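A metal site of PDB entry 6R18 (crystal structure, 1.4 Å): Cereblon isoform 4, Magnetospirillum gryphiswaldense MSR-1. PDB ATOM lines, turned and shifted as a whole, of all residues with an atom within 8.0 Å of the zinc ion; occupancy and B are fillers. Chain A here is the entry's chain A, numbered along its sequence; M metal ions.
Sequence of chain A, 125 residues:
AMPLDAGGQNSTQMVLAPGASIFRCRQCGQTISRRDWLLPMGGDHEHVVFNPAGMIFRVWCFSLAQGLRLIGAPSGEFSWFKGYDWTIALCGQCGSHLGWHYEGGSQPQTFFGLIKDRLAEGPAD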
ATOM      1  N   ARG A  24     -18.582 -22.748   9.132  1.00  0.00           N
ATOM      2  CA  ARG A  24     -17.682 -23.700   8.511  1.00  0.00           C
ATOM      3  C   ARG A  24     -17.946 -25.108   9.015  1.00  0.00           C
ATOM      4  O   ARG A  24     -18.460 -25.313  10.098  1.00  0.00           O
ATOM      5  CB  ARG A  24     -16.239 -23.276   8.841  1.00  0.00           C
ATOM      6  CG  ARG A  24     -15.861 -22.006   8.258  1.00  0.00           C
ATOM      7  CD  ARG A  24     -14.363 -21.638   8.466  1.00  0.00           C
ATOM      8  NE  ARG A  24     -14.011 -20.433   7.811  1.00  0.00           N
ATOM      9  CZ  ARG A  24     -13.832 -20.303   6.515  1.00  0.00           C
ATOM     10  NH1 ARG A  24     -13.732 -21.355   5.719  1.00  0.00           N
ATOM     11  NH2 ARG A  24     -13.685 -19.087   5.980  1.00  0.00           N
ATOM     12  N   CYS A  25     -17.560 -26.097   8.216  1.00  0.00           N
ATOM     13  CA  CYS A  25     -17.559 -27.493   8.672  1.00  0.00           C
ATOM     14  C   CYS A  25     -16.711 -27.600   9.934  1.00  0.00           C
ATOM     15  O   CYS A  25     -15.536 -27.209   9.936  1.00  0.00           O
ATOM     16  CB  CYS A  25     -17.071 -28.414   7.593  1.00  0.00           C
ATOM     17  SG  CYS A  25     -16.948 -30.119   8.147  1.00  0.00           S
ATOM     18  N   ARG A  26     -17.281 -28.155  11.009  1.00  0.00           N
ATOM     19  CA  ARG A  26     -16.527 -28.335  12.247  1.00  0.00           C
ATOM     20  C   ARG A  26     -15.340 -29.248  12.087  1.00  0.00           C
ATOM     21  O   ARG A  26     -14.350 -29.112  12.831  1.00  0.00           O
ATOM     22  CB  ARG A  26     -17.482 -28.860  13.325  1.00  0.00           C
ATOM     23  CG  ARG A  26     -16.854 -29.147  14.651  1.00  0.00           C
ATOM     24  CD  ARG A  26     -17.897 -29.580  15.604  1.00  0.00           C
ATOM     25  NE  ARG A  26     -17.303 -30.002  16.850  1.00  0.00           N
ATOM     26  CZ  ARG A  26     -17.951 -30.430  17.907  1.00  0.00           C
ATOM     27  NH1 ARG A  26     -19.253 -30.453  17.959  1.00  0.00           N
ATOM     28  NH2 ARG A  26     -17.265 -30.872  18.935  1.00  0.00           N
ATOM     29  N   GLN A  27     -15.415 -30.230  11.192  1.00  0.00           N
ATOM     30  CA  GLN A  27     -14.362 -31.231  11.069  1.00  0.00           C
ATOM     31  C   GLN A  27     -13.217 -30.743  10.250  1.00  0.00           C
ATOM     32  O   GLN A  27     -12.089 -31.269  10.432  1.00  0.00           O
ATOM     33  CB  GLN A  27     -14.944 -32.499  10.522  1.00  0.00           C
ATOM     34  CG  GLN A  27     -15.916 -33.119  11.465  1.00  0.00           C
ATOM     35  CD  GLN A  27     -15.426 -33.307  12.871  1.00  0.00           C
ATOM     36  OE1 GLN A  27     -14.308 -33.750  13.082  1.00  0.00           O
ATOM     37  NE2 GLN A  27     -16.231 -32.888  13.859  1.00  0.00           N
ATOM     38  N   CYS A  28     -13.351 -29.832   9.292  1.00  0.00           N
ATOM     39  CA  CYS A  28     -12.294 -29.488   8.377  1.00  0.00           C
ATOM     40  C   CYS A  28     -12.137 -28.046   8.068  1.00  0.00           C
ATOM     41  O   CYS A  28     -11.154 -27.621   7.469  1.00  0.00           O
ATOM     42  CB  CYS A  28     -12.428 -30.304   7.083  1.00  0.00           C
ATOM     43  SG  CYS A  28     -13.747 -29.703   5.988  1.00  0.00           S
ATOM     44  N   GLY A  29     -13.147 -27.183   8.316  1.00  0.00           N
ATOM     45  CA  GLY A  29     -13.099 -25.809   7.980  1.00  0.00           C
ATOM     46  C   GLY A  29     -13.629 -25.318   6.674  1.00  0.00           C
ATOM     47  O   GLY A  29     -13.681 -24.112   6.413  1.00  0.00           O
ATOM     48  N   GLN A  30     -14.206 -26.218   5.866  1.00  0.00           N
ATOM     49  CA  GLN A  30     -14.843 -25.820   4.611  1.00  0.00           C
ATOM     50  C   GLN A  30     -15.912 -24.750   4.899  1.00  0.00           C
ATOM     51  O   GLN A  30     -16.710 -24.902   5.792  1.00  0.00           O
ATOM     52  CB  GLN A  30     -15.528 -27.054   4.021  1.00  0.00           C
ATOM     53  CG  GLN A  30     -16.365 -26.803   2.782  1.00  0.00           C
ATOM     54  CD  GLN A  30     -15.576 -26.851   1.513  1.00  0.00           C
ATOM     55  OE1 GLN A  30     -14.437 -26.319   1.437  1.00  0.00           O
ATOM     56  NE2 GLN A  30     -16.115 -27.524   0.506  1.00  0.00           N
ATOM     57  N   THR A  31     -15.924 -23.707   4.074  1.00  0.00           N
ATOM     58  CA  THR A  31     -16.975 -22.696   4.206  1.00  0.00           C
ATOM     59  C   THR A  31     -18.331 -23.304   3.788  1.00  0.00           C
ATOM     60  O   THR A  31     -18.390 -23.862   2.727  1.00  0.00           O
ATOM     61  CB  THR A  31     -16.667 -21.520   3.259  1.00  0.00           C
ATOM     62  OG1 THR A  31     -15.200 -21.268   3.243  1.00  0.00           O
ATOM     63  CG2 THR A  31     -17.505 -20.412   3.630  1.00  0.00           C
ATOM     64  N   ILE A  32     -19.360 -23.161   4.612  1.00  0.00           N
ATOM     65  CA  ILE A  32     -20.685 -23.762   4.367  1.00  0.00           C
ATOM     66  C   ILE A  32     -21.795 -22.719   4.289  1.00  0.00           C
ATOM     67  O   ILE A  32     -22.602 -22.784   3.354  1.00  0.00           O
ATOM     68  CB  ILE A  32     -21.034 -24.817   5.408  1.00  0.00           C
ATOM     69  CG1 ILE A  32     -19.988 -25.902   5.527  1.00  0.00           C
ATOM     70  CG2 ILE A  32     -22.388 -25.432   5.130  1.00  0.00           C
ATOM     71  CD1 ILE A  32     -19.781 -26.737   4.318  1.00  0.00           C
ATOM     72  N   GLY A  67     -20.259 -25.363  -0.512  1.00  0.00           N
ATOM     73  CA  GLY A  67     -19.257 -26.245   0.007  1.00  0.00           C
ATOM     74  C   GLY A  67     -19.716 -27.599   0.330  1.00  0.00           C
ATOM     75  O   GLY A  67     -18.956 -28.382   0.954  1.00  0.00           O
ATOM     76  N   LEU A  68     -20.953 -27.961  -0.002  1.00  0.00           N
ATOM     77  CA  LEU A  68     -21.536 -29.251   0.271  1.00  0.00           C
ATOM     78  C   LEU A  68     -21.448 -30.099  -0.949  1.00  0.00           C
ATOM     79  O   LEU A  68     -21.147 -29.631  -2.051  1.00  0.00           O
ATOM     80  CB  LEU A  68     -23.007 -29.107   0.706  1.00  0.00           C
ATOM     81  CG  LEU A  68     -23.180 -28.297   1.979  1.00  0.00           C
ATOM     82  CD1 LEU A  68     -24.613 -27.812   2.096  1.00  0.00           C
ATOM     83  CD2 LEU A  68     -22.778 -29.086   3.223  1.00  0.00           C
ATOM     84  N   LEU A  90     -23.435 -33.661   2.390  1.00  0.00           N
ATOM     85  CA  LEU A  90     -22.126 -33.905   3.024  1.00  0.00           C
ATOM     86  C   LEU A  90     -21.281 -32.678   2.850  1.00  0.00           C
ATOM     87  O   LEU A  90     -21.413 -31.937   1.853  1.00  0.00           O
ATOM     88  CB  LEU A  90     -21.433 -35.065   2.390  1.00  0.00           C
ATOM     89  CG  LEU A  90     -22.218 -36.382   2.360  1.00  0.00           C
ATOM     90  CD1 LEU A  90     -21.343 -37.462   1.752  1.00  0.00           C
ATOM     91  CD2 LEU A  90     -22.706 -36.798   3.751  1.00  0.00           C
ATOM     92  N   CYS A  91     -20.349 -32.461   3.774  1.00  0.00           N
ATOM     93  CA  CYS A  91     -19.264 -31.514   3.490  1.00  0.00           C
ATOM     94  C   CYS A  91     -18.552 -31.982   2.237  1.00  0.00           C
ATOM     95  O   CYS A  91     -18.125 -33.148   2.098  1.00  0.00           O
ATOM     96  CB  CYS A  91     -18.293 -31.534   4.645  1.00  0.00           C
ATOM     97  SG  CYS A  91     -16.861 -30.441   4.374  1.00  0.00           S
ATOM     98  N   GLY A  92     -18.428 -31.066   1.259  1.00  0.00           N
ATOM     99  CA  GLY A  92     -17.810 -31.418   0.012  1.00  0.00           C
ATOM    100  C   GLY A  92     -16.315 -31.620   0.115  1.00  0.00           C
ATOM    101  O   GLY A  92     -15.744 -32.204  -0.802  1.00  0.00           O
ATOM    102  N   GLN A  93     -15.724 -31.166   1.190  1.00  0.00           N
ATOM    103  CA  GLN A  93     -14.288 -31.332   1.396  1.00  0.00           C
ATOM    104  C   GLN A  93     -14.004 -32.649   2.120  1.00  0.00           C
ATOM    105  O   GLN A  93     -13.330 -33.509   1.577  1.00  0.00           O
ATOM    106  CB  GLN A  93     -13.753 -30.081   2.092  1.00  0.00           C
ATOM    107  CG  GLN A  93     -12.247 -30.120   2.341  1.00  0.00           C
ATOM    108  CD  GLN A  93     -11.714 -28.720   2.626  1.00  0.00           C
ATOM    109  OE1 GLN A  93     -11.253 -28.079   1.681  1.00  0.00           O
ATOM    110  NE2 GLN A  93     -11.847 -28.213   3.828  1.00  0.00           N
ATOM    111  N   CYS A  94     -14.589 -32.847   3.297  1.00  0.00           N
ATOM    112  CA  CYS A  94     -14.191 -33.983   4.175  1.00  0.00           C
ATOM    113  C   CYS A  94     -15.236 -35.098   4.229  1.00  0.00           C
ATOM    114  O   CYS A  94     -14.935 -36.143   4.780  1.00  0.00           O
ATOM    115  CB  CYS A  94     -13.859 -33.531   5.554  1.00  0.00           C
ATOM    116  SG  CYS A  94     -15.299 -33.178   6.617  1.00  0.00           S
ATOM    117  N   GLY A  95     -16.454 -34.871   3.734  1.00  0.00           N
ATOM    118  CA  GLY A  95     -17.485 -35.894   3.773  1.00  0.00           C
ATOM    119  C   GLY A  95     -18.320 -35.973   5.005  1.00  0.00           C
ATOM    120  O   GLY A  95     -19.231 -36.812   5.051  1.00  0.00           O
ATOM    121  N   SER A  96     -18.096 -35.151   6.005  1.00  0.00           N
ATOM    122  CA  SER A  96     -18.919 -35.104   7.228  1.00  0.00           C
ATOM    123  C   SER A  96     -20.369 -34.887   6.827  1.00  0.00           C
ATOM    124  O   SER A  96     -20.674 -34.064   5.964  1.00  0.00           O
ATOM    125  CB  SER A  96     -18.458 -33.953   8.129  1.00  0.00           C
ATOM    126  OG  SER A  96     -19.226 -33.800   9.276  1.00  0.00           O
ATOM    127  N   HIS A  97     -21.281 -35.587   7.487  1.00  0.00           N
ATOM    128  CA  HIS A  97     -22.701 -35.382   7.196  1.00  0.00           C
ATOM    129  C   HIS A  97     -23.145 -34.116   7.900  1.00  0.00           C
ATOM    130  O   HIS A  97     -23.302 -34.076   9.109  1.00  0.00           O
ATOM    131  CB  HIS A  97     -23.523 -36.589   7.632  1.00  0.00           C
ATOM    132  CG  HIS A  97     -24.953 -36.364   7.424  1.00  0.00           C
ATOM    133  ND1 HIS A  97     -25.894 -37.014   8.190  1.00  0.00           N
ATOM    134  CD2 HIS A  97     -25.641 -35.599   6.532  1.00  0.00           C
ATOM    135  CE1 HIS A  97     -27.096 -36.603   7.787  1.00  0.00           C
ATOM    136  NE2 HIS A  97     -26.966 -35.755   6.797  1.00  0.00           N
ATOM    137  N   LEU A  98     -23.401 -33.038   7.144  1.00  0.00           N
ATOM    138  CA  LEU A  98     -23.779 -31.757   7.691  1.00  0.00           C
ATOM    139  C   LEU A  98     -25.260 -31.463   7.735  1.00  0.00           C
ATOM    140  O   LEU A  98     -25.673 -30.603   8.458  1.00  0.00           O
ATOM    141  CB  LEU A  98     -23.072 -30.634   6.948  1.00  0.00           C
ATOM    142  CG  LEU A  98     -21.533 -30.676   7.094  1.00  0.00           C
ATOM    143  CD1 LEU A  98     -20.912 -29.439   6.471  1.00  0.00           C
ATOM    144  CD2 LEU A  98     -21.038 -30.823   8.539  1.00  0.00           C
ATOM    145  N   ARG A 118     -22.611 -29.568  14.101  1.00  0.00           N
ATOM    146  CA  ARG A 118     -21.607 -30.010  13.130  1.00  0.00           C
ATOM    147  C   ARG A 118     -20.950 -28.882  12.368  1.00  0.00           C
ATOM    148  O   ARG A 118     -20.137 -29.106  11.443  1.00  0.00           O
ATOM    149  CB  ARG A 118     -22.226 -31.042  12.188  1.00  0.00           C
ATOM    150  CG  ARG A 118     -22.744 -32.250  12.992  1.00  0.00           C
ATOM    151  CD  ARG A 118     -23.154 -33.405  12.200  1.00  0.00           C
ATOM    152  NE  ARG A 118     -23.774 -34.433  13.005  1.00  0.00           N
ATOM    153  CZ  ARG A 118     -24.174 -35.594  12.526  1.00  0.00           C
ATOM    154  NH1 ARG A 118     -24.041 -35.905  11.274  1.00  0.00           N
ATOM    155  NH2 ARG A 118     -24.723 -36.504  13.322  1.00  0.00           N
HETATM  156 ZN    ZN M   1     -15.696 -30.886   6.352  1.00  0.00          ZN
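The side-chain sulfur (SG) of Cys 28 lies close to the backbone NH (N) of Gln 30 (3.5 Å). The side-chain amide nitrogen (NE2) of Gln 93 lies close to the side-chain sulfur (SG) of Cys 28 (3.2 Å). The backbone NH (N) of Cys 25 is in hydrogen-bond range of the backbone carbonyl oxygen (O) of Gln 30, 2.8 Å away. SG of Cys 25 lies close to N of Gln 27 (3.4 Å). The backbone carbonyl oxygen (O) of Ser 96 lies within hydrogen-bond range of the backbone NH (N) of Cys 91, at 2.7 Å. N of Gln 93 sits close to SG of Cys 91, at 3.5 Å. The backbone NH (N) of Ser 96 lies close to the side-chain sulfur (SG) of Cys 94 (3.5 Å).
SG of Cys 28 binds the zinc ion, 2.3 Å away. SG of Cys 25 binds the zinc ion (2.3 Å). SG of Cys 91 binds the zinc ion (2.3 Å). SG of Cys 94 binds the zinc ion (2.3 Å). The zinc ion has four donor atoms within binding distance.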
